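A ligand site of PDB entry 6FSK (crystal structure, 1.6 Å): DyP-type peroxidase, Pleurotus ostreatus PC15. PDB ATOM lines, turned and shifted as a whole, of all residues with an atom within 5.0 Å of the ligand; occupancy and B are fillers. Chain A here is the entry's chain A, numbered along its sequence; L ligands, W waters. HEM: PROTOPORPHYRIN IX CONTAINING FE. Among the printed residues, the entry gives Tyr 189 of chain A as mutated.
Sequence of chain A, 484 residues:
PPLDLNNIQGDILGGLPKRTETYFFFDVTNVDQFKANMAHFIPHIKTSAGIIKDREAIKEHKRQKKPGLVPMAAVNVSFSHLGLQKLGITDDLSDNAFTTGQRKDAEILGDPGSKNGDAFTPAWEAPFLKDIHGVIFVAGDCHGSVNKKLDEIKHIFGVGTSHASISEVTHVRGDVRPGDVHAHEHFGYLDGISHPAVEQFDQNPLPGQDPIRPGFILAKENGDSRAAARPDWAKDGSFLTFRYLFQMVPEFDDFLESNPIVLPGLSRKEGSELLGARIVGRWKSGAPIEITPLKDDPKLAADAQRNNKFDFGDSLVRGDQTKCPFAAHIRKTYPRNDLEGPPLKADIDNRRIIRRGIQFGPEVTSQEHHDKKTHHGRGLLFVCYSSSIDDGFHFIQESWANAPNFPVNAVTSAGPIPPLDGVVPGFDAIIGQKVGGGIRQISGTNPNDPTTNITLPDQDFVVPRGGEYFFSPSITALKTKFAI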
ATOM      1  N   GLU A 185     -11.832 -17.711   8.297  1.00  0.00           N
ATOM      2  CA  GLU A 185     -10.972 -16.691   7.636  1.00  0.00           C
ATOM      3  C   GLU A 185     -10.309 -17.294   6.413  1.00  0.00           C
ATOM      4  O   GLU A 185     -10.377 -18.513   6.255  1.00  0.00           O
ATOM      5  CB  GLU A 185     -10.063 -16.012   8.628  1.00  0.00           C
ATOM      6  CG  GLU A 185      -9.162 -16.961   9.365  1.00  0.00           C
ATOM      7  CD  GLU A 185      -8.165 -17.539   8.492  1.00  0.00           C
ATOM      8  OE1 GLU A 185      -7.871 -18.758   8.603  1.00  0.00           O
ATOM      9  OE2 GLU A 185      -7.527 -16.804   7.649  1.00  0.00           O
ATOM     10  N   PHE A 187      -7.380 -18.127   5.307  1.00  0.00           N
ATOM     11  CA  PHE A 187      -6.453 -19.249   5.406  1.00  0.00           C
ATOM     12  C   PHE A 187      -7.143 -20.558   5.661  1.00  0.00           C
ATOM     13  O   PHE A 187      -6.519 -21.622   5.485  1.00  0.00           O
ATOM     14  CB  PHE A 187      -5.323 -19.086   6.424  1.00  0.00           C
ATOM     15  CG  PHE A 187      -4.396 -17.913   6.196  1.00  0.00           C
ATOM     16  CD1 PHE A 187      -3.804 -17.619   4.984  1.00  0.00           C
ATOM     17  CD2 PHE A 187      -4.073 -17.088   7.256  1.00  0.00           C
ATOM     18  CE1 PHE A 187      -2.943 -16.530   4.854  1.00  0.00           C
ATOM     19  CE2 PHE A 187      -3.253 -15.987   7.134  1.00  0.00           C
ATOM     20  CZ  PHE A 187      -2.724 -15.657   5.878  1.00  0.00           C
ATOM     21  N   TYR A 189      -9.313 -21.195   8.636  1.00  0.00           N
ATOM     22  CA  TYR A 189      -9.472 -21.540  10.079  1.00  0.00           C
ATOM     23  C   TYR A 189     -10.747 -20.888  10.574  1.00  0.00           C
ATOM     24  O   TYR A 189     -11.008 -19.699  10.325  1.00  0.00           O
ATOM     25  CB  TYR A 189      -8.274 -21.052  10.876  1.00  0.00           C
ATOM     26  CG  TYR A 189      -7.069 -21.883  10.522  1.00  0.00           C
ATOM     27  CD1 TYR A 189      -6.327 -21.565   9.416  1.00  0.00           C
ATOM     28  CD2 TYR A 189      -6.648 -22.959  11.293  1.00  0.00           C
ATOM     29  CE1 TYR A 189      -5.278 -22.367   8.940  1.00  0.00           C
ATOM     30  CE2 TYR A 189      -5.614 -23.754  10.856  1.00  0.00           C
ATOM     31  CZ  TYR A 189      -4.934 -23.469   9.693  1.00  0.00           C
ATOM     32  OH  TYR A 189      -3.845 -24.220   9.185  1.00  0.00           O
ATOM     33  N   LEU A 190     -11.600 -21.611  11.289  1.00  0.00           N
ATOM     34  CA  LEU A 190     -12.790 -21.014  11.916  1.00  0.00           C
ATOM     35  C   LEU A 190     -12.357 -19.882  12.833  1.00  0.00           C
ATOM     36  O   LEU A 190     -11.452 -19.990  13.607  1.00  0.00           O
ATOM     37  CB  LEU A 190     -13.553 -22.088  12.693  1.00  0.00           C
ATOM     38  CG  LEU A 190     -14.792 -21.611  13.477  1.00  0.00           C
ATOM     39  CD1 LEU A 190     -15.777 -21.144  12.402  1.00  0.00           C
ATOM     40  CD2 LEU A 190     -15.410 -22.755  14.281  1.00  0.00           C
ATOM     41  N   ASP A 191     -12.997 -18.712  12.683  1.00  0.00           N
ATOM     42  CA  ASP A 191     -12.629 -17.468  13.362  1.00  0.00           C
ATOM     43  C   ASP A 191     -13.850 -17.011  14.133  1.00  0.00           C
ATOM     44  O   ASP A 191     -14.986 -17.325  13.779  1.00  0.00           O
ATOM     45  CB  ASP A 191     -12.282 -16.437  12.262  1.00  0.00           C
ATOM     46  CG  ASP A 191     -11.491 -15.203  12.775  1.00  0.00           C
ATOM     47  OD1 ASP A 191     -10.928 -15.198  13.875  1.00  0.00           O
ATOM     48  OD2 ASP A 191     -11.469 -14.201  12.009  1.00  0.00           O
ATOM     49  N   GLY A 192     -13.603 -16.303  15.196  1.00  0.00           N
ATOM     50  CA  GLY A 192     -14.705 -15.796  16.016  1.00  0.00           C
ATOM     51  C   GLY A 192     -15.090 -16.612  17.220  1.00  0.00           C
ATOM     52  O   GLY A 192     -16.195 -16.479  17.691  1.00  0.00           O
ATOM     53  N   ILE A 193     -14.226 -17.507  17.687  1.00  0.00           N
ATOM     54  CA  ILE A 193     -14.568 -18.490  18.682  1.00  0.00           C
ATOM     55  C   ILE A 193     -14.425 -17.863  20.072  1.00  0.00           C
ATOM     56  O   ILE A 193     -15.278 -17.995  20.946  1.00  0.00           O
ATOM     57  CB  ILE A 193     -13.689 -19.744  18.569  1.00  0.00           C
ATOM     58  CG1 ILE A 193     -13.899 -20.377  17.168  1.00  0.00           C
ATOM     59  CG2 ILE A 193     -13.887 -20.717  19.727  1.00  0.00           C
ATOM     60  CD1 ILE A 193     -12.912 -21.446  16.808  1.00  0.00           C
ATOM     61  N   SER A 194     -13.218 -17.324  20.325  1.00  0.00           N
ATOM     62  CA  SER A 194     -12.869 -16.935  21.682  1.00  0.00           C
ATOM     63  C   SER A 194     -12.906 -15.434  21.911  1.00  0.00           C
ATOM     64  O   SER A 194     -12.055 -14.716  21.391  1.00  0.00           O
ATOM     65  CB  SER A 194     -11.482 -17.483  22.105  1.00  0.00           C
ATOM     66  OG  SER A 194     -11.141 -17.145  23.466  1.00  0.00           O
ATOM     67  N   LEU A 245      -6.244  -6.021   6.435  1.00  0.00           N
ATOM     68  CA  LEU A 245      -5.194  -7.082   6.440  1.00  0.00           C
ATOM     69  C   LEU A 245      -5.305  -7.999   5.257  1.00  0.00           C
ATOM     70  O   LEU A 245      -6.197  -8.820   5.192  1.00  0.00           O
ATOM     71  CB  LEU A 245      -5.183  -7.865   7.730  1.00  0.00           C
ATOM     72  CG  LEU A 245      -4.901  -7.011   8.959  1.00  0.00           C
ATOM     73  CD1 LEU A 245      -4.963  -7.930  10.228  1.00  0.00           C
ATOM     74  CD2 LEU A 245      -3.575  -6.290   8.984  1.00  0.00           C
ATOM     75  N   GLN A 247      -4.393 -11.135   2.982  1.00  0.00           N
ATOM     76  CA  GLN A 247      -3.828 -12.450   3.233  1.00  0.00           C
ATOM     77  C   GLN A 247      -3.316 -13.069   1.927  1.00  0.00           C
ATOM     78  O   GLN A 247      -3.971 -13.026   0.911  1.00  0.00           O
ATOM     79  CB  GLN A 247      -4.885 -13.335   3.846  1.00  0.00           C
ATOM     80  CG  GLN A 247      -5.231 -12.834   5.265  1.00  0.00           C
ATOM     81  CD  GLN A 247      -6.391 -13.600   5.834  1.00  0.00           C
ATOM     82  OE1 GLN A 247      -7.408 -13.014   6.092  1.00  0.00           O
ATOM     83  NE2 GLN A 247      -6.237 -14.820   6.177  1.00  0.00           N
ATOM     84  N   VAL A 280      -1.469 -21.847  14.257  1.00  0.00           N
ATOM     85  CA  VAL A 280      -2.651 -21.073  14.675  1.00  0.00           C
ATOM     86  C   VAL A 280      -2.978 -21.319  16.127  1.00  0.00           C
ATOM     87  O   VAL A 280      -3.321 -20.416  16.889  1.00  0.00           O
ATOM     88  CB  VAL A 280      -3.834 -21.432  13.771  1.00  0.00           C
ATOM     89  CG1 VAL A 280      -5.107 -20.743  14.305  1.00  0.00           C
ATOM     90  CG2 VAL A 280      -3.541 -20.977  12.365  1.00  0.00           C
ATOM     91  N   ARG A 282      -5.254 -23.883  16.556  1.00  0.00           N
ATOM     92  CA  ARG A 282      -6.473 -24.651  16.285  1.00  0.00           C
ATOM     93  C   ARG A 282      -6.375 -25.276  14.955  1.00  0.00           C
ATOM     94  O   ARG A 282      -5.744 -24.688  14.064  1.00  0.00           O
ATOM     95  CB  ARG A 282      -7.756 -23.763  16.341  1.00  0.00           C
ATOM     96  CG  ARG A 282      -8.071 -23.064  17.642  1.00  0.00           C
ATOM     97  CD  ARG A 282      -9.315 -22.219  17.566  1.00  0.00           C
ATOM     98  NE  ARG A 282      -9.569 -21.548  18.811  1.00  0.00           N
ATOM     99  CZ  ARG A 282     -10.238 -22.095  19.848  1.00  0.00           C
ATOM    100  NH1 ARG A 282     -10.888 -23.239  19.758  1.00  0.00           N
ATOM    101  NH2 ARG A 282     -10.360 -21.420  20.942  1.00  0.00           N
ATOM    102  N   ASN A 308     -13.416 -24.147  23.878  1.00  0.00           N
ATOM    103  CA  ASN A 308     -12.567 -23.091  24.438  1.00  0.00           C
ATOM    104  C   ASN A 308     -12.141 -23.305  25.873  1.00  0.00           C
ATOM    105  O   ASN A 308     -11.627 -22.429  26.532  1.00  0.00           O
ATOM    106  CB  ASN A 308     -13.235 -21.745  24.127  1.00  0.00           C
ATOM    107  CG  ASN A 308     -12.230 -20.613  24.113  1.00  0.00           C
ATOM    108  OD1 ASN A 308     -11.136 -20.773  23.619  1.00  0.00           O
ATOM    109  ND2 ASN A 308     -12.663 -19.481  24.586  1.00  0.00           N
ATOM    110  N   HIS A 329      -0.565 -18.642  17.261  1.00  0.00           N
ATOM    111  CA  HIS A 329      -1.242 -17.329  17.237  1.00  0.00           C
ATOM    112  C   HIS A 329      -2.146 -17.059  18.384  1.00  0.00           C
ATOM    113  O   HIS A 329      -2.078 -16.035  19.001  1.00  0.00           O
ATOM    114  CB  HIS A 329      -1.977 -17.220  15.945  1.00  0.00           C
ATOM    115  CG  HIS A 329      -2.798 -15.991  15.816  1.00  0.00           C
ATOM    116  ND1 HIS A 329      -2.277 -14.728  15.880  1.00  0.00           N
ATOM    117  CD2 HIS A 329      -4.125 -15.832  15.579  1.00  0.00           C
ATOM    118  CE1 HIS A 329      -3.248 -13.846  15.667  1.00  0.00           C
ATOM    119  NE2 HIS A 329      -4.384 -14.491  15.559  1.00  0.00           N
ATOM    120  N   ILE A 330      -2.949 -18.038  18.745  1.00  0.00           N
ATOM    121  CA  ILE A 330      -3.931 -17.747  19.814  1.00  0.00           C
ATOM    122  C   ILE A 330      -3.221 -17.587  21.147  1.00  0.00           C
ATOM    123  O   ILE A 330      -3.728 -16.937  22.052  1.00  0.00           O
ATOM    124  CB  ILE A 330      -5.080 -18.814  19.973  1.00  0.00           C
ATOM    125  CG1 ILE A 330      -4.569 -20.168  20.504  1.00  0.00           C
ATOM    126  CG2 ILE A 330      -5.834 -18.903  18.661  1.00  0.00           C
ATOM    127  CD1 ILE A 330      -5.690 -21.173  20.772  1.00  0.00           C
ATOM    128  N   THR A 333      -1.712 -14.148  21.485  1.00  0.00           N
ATOM    129  CA  THR A 333      -2.683 -13.078  21.561  1.00  0.00           C
ATOM    130  C   THR A 333      -3.593 -13.176  22.801  1.00  0.00           C
ATOM    131  O   THR A 333      -3.999 -12.147  23.289  1.00  0.00           O
ATOM    132  CB  THR A 333      -3.544 -12.974  20.291  1.00  0.00           C
ATOM    133  OG1 THR A 333      -4.270 -14.186  20.107  1.00  0.00           O
ATOM    134  CG2 THR A 333      -2.684 -12.600  19.026  1.00  0.00           C
ATOM    135  N   TYR A 334      -3.759 -14.362  23.323  1.00  0.00           N
ATOM    136  CA  TYR A 334      -4.384 -14.533  24.652  1.00  0.00           C
ATOM    137  C   TYR A 334      -3.577 -15.626  25.379  1.00  0.00           C
ATOM    138  O   TYR A 334      -3.842 -16.827  25.240  1.00  0.00           O
ATOM    139  CB  TYR A 334      -5.838 -14.892  24.586  1.00  0.00           C
ATOM    140  CG  TYR A 334      -6.507 -15.142  25.930  1.00  0.00           C
ATOM    141  CD1 TYR A 334      -6.095 -14.497  27.046  1.00  0.00           C
ATOM    142  CD2 TYR A 334      -7.590 -15.994  26.010  1.00  0.00           C
ATOM    143  CE1 TYR A 334      -6.726 -14.770  28.281  1.00  0.00           C
ATOM    144  CE2 TYR A 334      -8.216 -16.253  27.188  1.00  0.00           C
ATOM    145  CZ  TYR A 334      -7.791 -15.619  28.301  1.00  0.00           C
ATOM    146  OH  TYR A 334      -8.442 -15.970  29.517  1.00  0.00           O
ATOM    147  N   ARG A 336      -3.501 -16.865  28.353  1.00  0.00           N
ATOM    148  CA  ARG A 336      -4.090 -17.728  29.386  1.00  0.00           C
ATOM    149  C   ARG A 336      -3.133 -17.968  30.535  1.00  0.00           C
ATOM    150  O   ARG A 336      -2.514 -17.018  31.074  1.00  0.00           O
ATOM    151  CB  ARG A 336      -4.690 -19.025  28.785  1.00  0.00           C
ATOM    152  CG  ARG A 336      -5.651 -18.680  27.588  1.00  0.00           C
ATOM    153  CD  ARG A 336      -6.419 -19.896  27.080  1.00  0.00           C
ATOM    154  NE  ARG A 336      -7.077 -19.582  25.815  1.00  0.00           N
ATOM    155  CZ  ARG A 336      -8.290 -19.913  25.480  1.00  0.00           C
ATOM    156  NH1 ARG A 336      -9.000 -20.729  26.256  1.00  0.00           N
ATOM    157  NH2 ARG A 336      -8.795 -19.438  24.354  1.00  0.00           N
ATOM    158  N   ARG A 352      -7.367  -7.874  26.970  1.00  0.00           N
ATOM    159  CA  ARG A 352      -8.418  -8.545  26.233  1.00  0.00           C
ATOM    160  C   ARG A 352      -9.023  -7.590  25.216  1.00  0.00           C
ATOM    161  O   ARG A 352      -9.101  -6.378  25.442  1.00  0.00           O
ATOM    162  CB  ARG A 352      -9.513  -9.102  27.176  1.00  0.00           C
ATOM    163  CG  ARG A 352      -8.923 -10.056  28.196  1.00  0.00           C
ATOM    164  CD  ARG A 352      -8.216 -11.247  27.657  1.00  0.00           C
ATOM    165  NE  ARG A 352      -9.044 -12.077  26.753  1.00  0.00           N
ATOM    166  CZ  ARG A 352      -9.887 -12.994  27.111  1.00  0.00           C
ATOM    167  NH1 ARG A 352     -10.163 -13.233  28.440  1.00  0.00           N
ATOM    168  NH2 ARG A 352     -10.553 -13.651  26.195  1.00  0.00           N
ATOM    169  N   ILE A 353      -9.488  -8.183  24.113  1.00  0.00           N
ATOM    170  CA  ILE A 353     -10.158  -7.453  23.052  1.00  0.00           C
ATOM    171  C   ILE A 353     -11.318  -8.215  22.541  1.00  0.00           C
ATOM    172  O   ILE A 353     -11.352  -9.453  22.591  1.00  0.00           O
ATOM    173  CB  ILE A 353      -9.168  -7.141  21.853  1.00  0.00           C
ATOM    174  CG1 ILE A 353      -8.624  -8.458  21.230  1.00  0.00           C
ATOM    175  CG2 ILE A 353      -8.059  -6.229  22.285  1.00  0.00           C
ATOM    176  CD1 ILE A 353      -7.818  -8.192  19.972  1.00  0.00           C
ATOM    177  N   ARG A 355     -13.239  -8.935  19.147  1.00  0.00           N
ATOM    178  CA  ARG A 355     -13.031  -8.841  17.666  1.00  0.00           C
ATOM    179  C   ARG A 355     -14.308  -8.945  16.901  1.00  0.00           C
ATOM    180  O   ARG A 355     -15.222  -9.736  17.239  1.00  0.00           O
ATOM    181  CB  ARG A 355     -12.105  -9.950  17.212  1.00  0.00           C
ATOM    182  CG  ARG A 355     -10.724  -9.813  17.732  1.00  0.00           C
ATOM    183  CD  ARG A 355      -9.890 -11.080  17.575  1.00  0.00           C
ATOM    184  NE  ARG A 355     -10.452 -12.196  18.358  1.00  0.00           N
ATOM    185  CZ  ARG A 355     -10.756 -13.374  17.826  1.00  0.00           C
ATOM    186  NH1 ARG A 355     -10.502 -13.669  16.534  1.00  0.00           N
ATOM    187  NH2 ARG A 355     -11.317 -14.265  18.570  1.00  0.00           N
ATOM    188  N   LEU A 380      -8.823  -9.953   5.674  1.00  0.00           N
ATOM    189  CA  LEU A 380      -9.637  -9.700   6.849  1.00  0.00           C
ATOM    190  C   LEU A 380      -9.732  -8.186   7.075  1.00  0.00           C
ATOM    191  O   LEU A 380      -8.727  -7.479   7.117  1.00  0.00           O
ATOM    192  CB  LEU A 380      -9.021 -10.381   8.082  1.00  0.00           C
ATOM    193  CG  LEU A 380      -9.806 -10.367   9.353  1.00  0.00           C
ATOM    194  CD1 LEU A 380     -11.045 -11.216   9.237  1.00  0.00           C
ATOM    195  CD2 LEU A 380      -8.916 -10.913  10.480  1.00  0.00           C
ATOM    196  N   PHE A 382     -10.000  -6.439   9.862  1.00  0.00           N
ATOM    197  CA  PHE A 382      -9.826  -6.680  11.302  1.00  0.00           C
ATOM    198  C   PHE A 382     -10.388  -5.463  12.056  1.00  0.00           C
ATOM    199  O   PHE A 382      -9.984  -4.361  11.810  1.00  0.00           O
ATOM    200  CB  PHE A 382      -8.346  -6.835  11.636  1.00  0.00           C
ATOM    201  CG  PHE A 382      -8.082  -7.001  13.081  1.00  0.00           C
ATOM    202  CD1 PHE A 382      -8.036  -8.255  13.677  1.00  0.00           C
ATOM    203  CD2 PHE A 382      -7.814  -5.919  13.842  1.00  0.00           C
ATOM    204  CE1 PHE A 382      -7.837  -8.373  15.066  1.00  0.00           C
ATOM    205  CE2 PHE A 382      -7.527  -6.060  15.206  1.00  0.00           C
ATOM    206  CZ  PHE A 382      -7.561  -7.289  15.797  1.00  0.00           C
ATOM    207  N   PHE A 393      -4.851  -3.855  21.725  1.00  0.00           N
ATOM    208  CA  PHE A 393      -4.315  -4.092  20.390  1.00  0.00           C
ATOM    209  C   PHE A 393      -2.844  -3.745  20.222  1.00  0.00           C
ATOM    210  O   PHE A 393      -2.065  -4.530  19.713  1.00  0.00           O
ATOM    211  CB  PHE A 393      -5.126  -3.324  19.341  1.00  0.00           C
ATOM    212  CG  PHE A 393      -4.448  -3.356  17.993  1.00  0.00           C
ATOM    213  CD1 PHE A 393      -4.576  -4.502  17.182  1.00  0.00           C
ATOM    214  CD2 PHE A 393      -3.650  -2.282  17.584  1.00  0.00           C
ATOM    215  CE1 PHE A 393      -3.866  -4.588  15.989  1.00  0.00           C
ATOM    216  CE2 PHE A 393      -2.938  -2.366  16.356  1.00  0.00           C
ATOM    217  CZ  PHE A 393      -3.054  -3.525  15.577  1.00  0.00           C
ATOM    218  N   ILE A 396      -0.515  -6.128  22.286  1.00  0.00           N
ATOM    219  CA  ILE A 396      -0.563  -7.441  21.770  1.00  0.00           C
ATOM    220  C   ILE A 396       0.359  -7.537  20.555  1.00  0.00           C
ATOM    221  O   ILE A 396       1.125  -8.512  20.435  1.00  0.00           O
ATOM    222  CB  ILE A 396      -1.974  -7.886  21.351  1.00  0.00           C
ATOM    223  CG1 ILE A 396      -2.943  -8.049  22.558  1.00  0.00           C
ATOM    224  CG2 ILE A 396      -1.985  -9.213  20.590  1.00  0.00           C
ATOM    225  CD1 ILE A 396      -4.428  -8.042  22.191  1.00  0.00           C
ATOM    226  N   GLN A 397       0.187  -6.603  19.636  1.00  0.00           N
ATOM    227  CA  GLN A 397       0.993  -6.623  18.440  1.00  0.00           C
ATOM    228  C   GLN A 397       2.448  -6.492  18.731  1.00  0.00           C
ATOM    229  O   GLN A 397       3.279  -7.315  18.282  1.00  0.00           O
ATOM    230  CB  GLN A 397       0.538  -5.533  17.510  1.00  0.00           C
ATOM    231  CG  GLN A 397       1.246  -5.502  16.112  1.00  0.00           C
ATOM    232  CD  GLN A 397       0.773  -6.653  15.214  1.00  0.00           C
ATOM    233  OE1 GLN A 397      -0.384  -6.802  14.950  1.00  0.00           O
ATOM    234  NE2 GLN A 397       1.703  -7.538  14.858  1.00  0.00           N
ATOM    235  N   ILE A 430       1.329 -15.724  11.996  1.00  0.00           N
ATOM    236  CA  ILE A 430       0.179 -15.165  11.275  1.00  0.00           C
ATOM    237  C   ILE A 430       0.296 -13.637  11.186  1.00  0.00           C
ATOM    238  O   ILE A 430       0.239 -13.051  10.137  1.00  0.00           O
ATOM    239  CB  ILE A 430      -1.167 -15.576  11.934  1.00  0.00           C
ATOM    240  CG1 ILE A 430      -1.269 -17.074  12.024  1.00  0.00           C
ATOM    241  CG2 ILE A 430      -2.342 -14.956  11.222  1.00  0.00           C
ATOM    242  CD1 ILE A 430      -1.330 -17.803  10.711  1.00  0.00           C
ATOM    243  N   ILE A 431       0.496 -12.993  12.323  1.00  0.00           N
ATOM    244  CA  ILE A 431       0.511 -11.533  12.404  1.00  0.00           C
ATOM    245  C   ILE A 431       1.817 -10.896  12.879  1.00  0.00           C
ATOM    246  O   ILE A 431       1.946  -9.685  12.846  1.00  0.00           O
ATOM    247  CB  ILE A 431      -0.648 -10.959  13.297  1.00  0.00           C
ATOM    248  CG1 ILE A 431      -0.507 -11.421  14.766  1.00  0.00           C
ATOM    249  CG2 ILE A 431      -2.003 -11.362  12.821  1.00  0.00           C
ATOM    250  CD1 ILE A 431      -1.202 -10.600  15.789  1.00  0.00           C
ATOM    251  N   VAL A 462       0.490 -12.141   6.007  1.00  0.00           N
ATOM    252  CA  VAL A 462      -0.526 -11.051   6.236  1.00  0.00           C
ATOM    253  C   VAL A 462       0.178  -9.752   5.978  1.00  0.00           C
ATOM    254  O   VAL A 462       1.282  -9.547   6.464  1.00  0.00           O
ATOM    255  CB  VAL A 462      -1.065 -11.147   7.715  1.00  0.00           C
ATOM    256  CG1 VAL A 462      -1.997  -9.960   7.947  1.00  0.00           C
ATOM    257  CG2 VAL A 462      -1.866 -12.411   7.857  1.00  0.00           C
HETATM  258  CHA HEM L   1      -7.847 -15.668  17.445  1.00  0.00           C
HETATM  259  CHB HEM L   1      -6.945 -15.621  12.712  1.00  0.00           C
HETATM  260  CHC HEM L   1      -5.342 -11.098  13.135  1.00  0.00           C
HETATM  261  CHD HEM L   1      -5.949 -11.247  17.939  1.00  0.00           C
HETATM  262  C1A HEM L   1      -7.763 -16.092  16.113  1.00  0.00           C
HETATM  263  C2A HEM L   1      -8.181 -17.356  15.607  1.00  0.00           C
HETATM  264  C3A HEM L   1      -7.978 -17.334  14.279  1.00  0.00           C
HETATM  265  C4A HEM L   1      -7.354 -16.079  13.987  1.00  0.00           C
HETATM  266  CMA HEM L   1      -8.195 -18.454  13.319  1.00  0.00           C
HETATM  267  CAA HEM L   1      -8.714 -18.508  16.446  1.00  0.00           C
HETATM  268  CBA HEM L   1     -10.219 -18.621  16.612  1.00  0.00           C
HETATM  269  CGA HEM L   1     -10.801 -17.523  17.482  1.00  0.00           C
HETATM  270  O1A HEM L   1     -10.658 -17.565  18.699  1.00  0.00           O
HETATM  271  O2A HEM L   1     -11.439 -16.611  16.905  1.00  0.00           O
HETATM  272  C1B HEM L   1      -6.409 -14.377  12.369  1.00  0.00           C
HETATM  273  C2B HEM L   1      -6.095 -13.933  11.088  1.00  0.00           C
HETATM  274  C3B HEM L   1      -5.664 -12.646  11.163  1.00  0.00           C
HETATM  275  C4B HEM L   1      -5.706 -12.313  12.595  1.00  0.00           C
HETATM  276  CMB HEM L   1      -6.165 -14.755   9.827  1.00  0.00           C
HETATM  277  CAB HEM L   1      -5.184 -11.668  10.144  1.00  0.00           C
HETATM  278  CBB HEM L   1      -5.472 -11.765   8.867  1.00  0.00           C
HETATM  279  C1C HEM L   1      -5.261 -10.721  14.435  1.00  0.00           C
HETATM  280  C2C HEM L   1      -4.765  -9.535  14.993  1.00  0.00           C
HETATM  281  C3C HEM L   1      -4.891  -9.554  16.352  1.00  0.00           C
HETATM  282  C4C HEM L   1      -5.576 -10.797  16.662  1.00  0.00           C
HETATM  283  CMC HEM L   1      -4.201  -8.407  14.175  1.00  0.00           C
HETATM  284  CAC HEM L   1      -4.468  -8.625  17.426  1.00  0.00           C
HETATM  285  CBC HEM L   1      -3.418  -7.779  17.322  1.00  0.00           C
HETATM  286  C1D HEM L   1      -6.589 -12.467  18.172  1.00  0.00           C
HETATM  287  C2D HEM L   1      -7.115 -12.795  19.528  1.00  0.00           C
HETATM  288  C3D HEM L   1      -7.697 -14.047  19.359  1.00  0.00           C
HETATM  289  C4D HEM L   1      -7.434 -14.425  17.972  1.00  0.00           C
HETATM  290  CMD HEM L   1      -7.094 -11.977  20.754  1.00  0.00           C
HETATM  291  CAD HEM L   1      -8.354 -14.927  20.416  1.00  0.00           C
HETATM  292  CBD HEM L   1      -7.372 -15.752  21.179  1.00  0.00           C
HETATM  293  CGD HEM L   1      -8.035 -16.507  22.299  1.00  0.00           C
HETATM  294  O1D HEM L   1      -7.758 -17.728  22.312  1.00  0.00           O
HETATM  295  O2D HEM L   1      -8.843 -15.957  23.022  1.00  0.00           O
HETATM  296  NA  HEM L   1      -7.147 -15.315  15.133  1.00  0.00           N
HETATM  297  NB  HEM L   1      -6.091 -13.420  13.284  1.00  0.00           N
HETATM  298  NC  HEM L   1      -5.638 -11.559  15.520  1.00  0.00           N
HETATM  299  ND  HEM L   1      -6.732 -13.489  17.330  1.00  0.00           N
HETATM  300 FE   HEM L   1      -6.343 -13.486  15.336  1.00  0.00          FE
HETATM  301  O   HOH W   1      -8.939 -12.736  14.184  1.00  0.00           O
HETATM  302  O   HOH W   2      -8.901 -19.050  20.195  1.00  0.00           O
HETATM  303  O   HOH W   3     -10.024 -13.513  23.275  1.00  0.00           O
HETATM  304  O   HOH W   4      -5.416 -18.625  23.731  1.00  0.00           O
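NE2 of His 329 binds FE of the ligand (2.2 Å). The backbone NH of Ser 194 is in hydrogen-bond range of an oxygen (O1A) of the ligand, at 3.0 Å. An oxygen (O2D) of the ligand sits at hydrogen-bond distance from the side-chain hydroxyl of Ser 194. The backbone NH (N) of Gly 192 sits at hydrogen-bond distance from an oxygen (O2A) of the ligand. O1D of the ligand is in salt-bridge range of NH2 of Arg 336 (2.9 Å). An oxygen (O2A) of the ligand lies within salt-bridge range of the guanidinium group (NH2) of Arg 355 (2.9 Å). The backbone NH (N) of Ile 193 lies within hydrogen-bond range of an oxygen (O2A) of the ligand (3.0 Å).
The backbone carbonyl oxygen of Ser 194 lies within hydrogen-bond range of the guanidinium group of Arg 355. The side-chain amide nitrogen of Asn 308 lies within hydrogen-bond range of the side-chain hydroxyl of Ser 194, 3.0 Å away. NH2 of Arg 336 is in hydrogen-bond range of OD1 of Asn 308 (2.8 Å). The backbone NH (N) of Tyr 189 lies within hydrogen-bond range of the side-chain carboxylate (OE1) of Glu 185. The side-chain amide nitrogen of Gln 247 lies within hydrogen-bond range of the side-chain carboxylate of Glu 185 (2.8 Å). The backbone NH (N) of Phe 187 lies within hydrogen-bond range of the side-chain carboxylate (OE2) of Glu 185, 2.7 Å away. NE2 of Gln 397 sits at hydrogen-bond distance from O of Ile 431, at 3.0 Å. O of Leu 245 is in hydrogen-bond range of N of Leu 380.
An oxygen (O2A) of the ligand lies close to the side-chain carboxylate (OD1) of Asp 191, at 3.4 Å. OE2 of Glu 185 touches CMB of the ligand, 3.3 Å away. Tyr 189 touches the ligand (CB to CMA, 3.6 Å). Leu 190 touches the ligand. Leu 245 touches the ligand (CD1 to CAB, 3.7 Å). OE1 of Gln 247 touches CBB of the ligand (3.6 Å). CG1 of Val 280 touches CMA of the ligand (3.97 Å). Arg 282 touches the ligand. Ile 330 touches the ligand. Thr 333 touches the ligand (OG1 to C2D, 3.2 Å). Tyr 334 touches the ligand (CD2 to O2D, 3.2 Å). Ile 353 touches the ligand (CG1 to CMD, 3.9 Å). CD2 of Leu 380 touches C3B of the ligand, at 3.7 Å. CE1 of Phe 382 touches C2C of the ligand (3.3 Å). Phe 393 touches the ligand (CD1 to CBC, 3.5 Å). Ile 396 touches the ligand (CG2 to CBC, 3.8 Å). OE1 of Gln 397 touches CBC of the ligand, at 3.97 Å. Ile 430 touches the ligand. CG2 of Ile 431 touches CHC of the ligand (3.4 Å). Val 462 touches the ligand. 26 residues have an atom within 4 Å of the ligand: Glu 185, Tyr 189, Leu 190, Asp 191, Gly 192, Ile 193, Ser 194, Leu 245, Gln 247, Val 280, Arg 282, His 329, Ile 330, Thr 333, Tyr 334, Arg 336, Ile 353, Arg 355, Leu 380, Phe 382, Phe 393, Ile 396, Gln 397, Ile 430, Ile 431 and Val 462. Along chain A the residues within 4 Å of the ligand span positions 185 to 462.
Water W3 lies within hydrogen-bond range of an oxygen (O2D) of the ligand (2.7 Å), the guanidinium group (NH2) of Arg 352 (3.0 Å) and the backbone carbonyl oxygen (O) of Ser 194 (3.0 Å). Water W2 lies within hydrogen-bond range of an oxygen (O1A) of the ligand and the guanidinium group of Arg 282. Water W4 lies within hydrogen-bond range of the backbone carbonyl oxygen (O) of Tyr 334 (2.8 Å), the guanidinium group (NE) of Arg 336 (2.8 Å), an oxygen (O1D) of the ligand (2.9 Å) and the backbone carbonyl oxygen (O) of Ile 330 (2.9 Å). Water W1 lies within hydrogen-bond range of NH1 of Arg 355 (3.0 Å) and OD1 of Asp 191 (3.2 Å).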
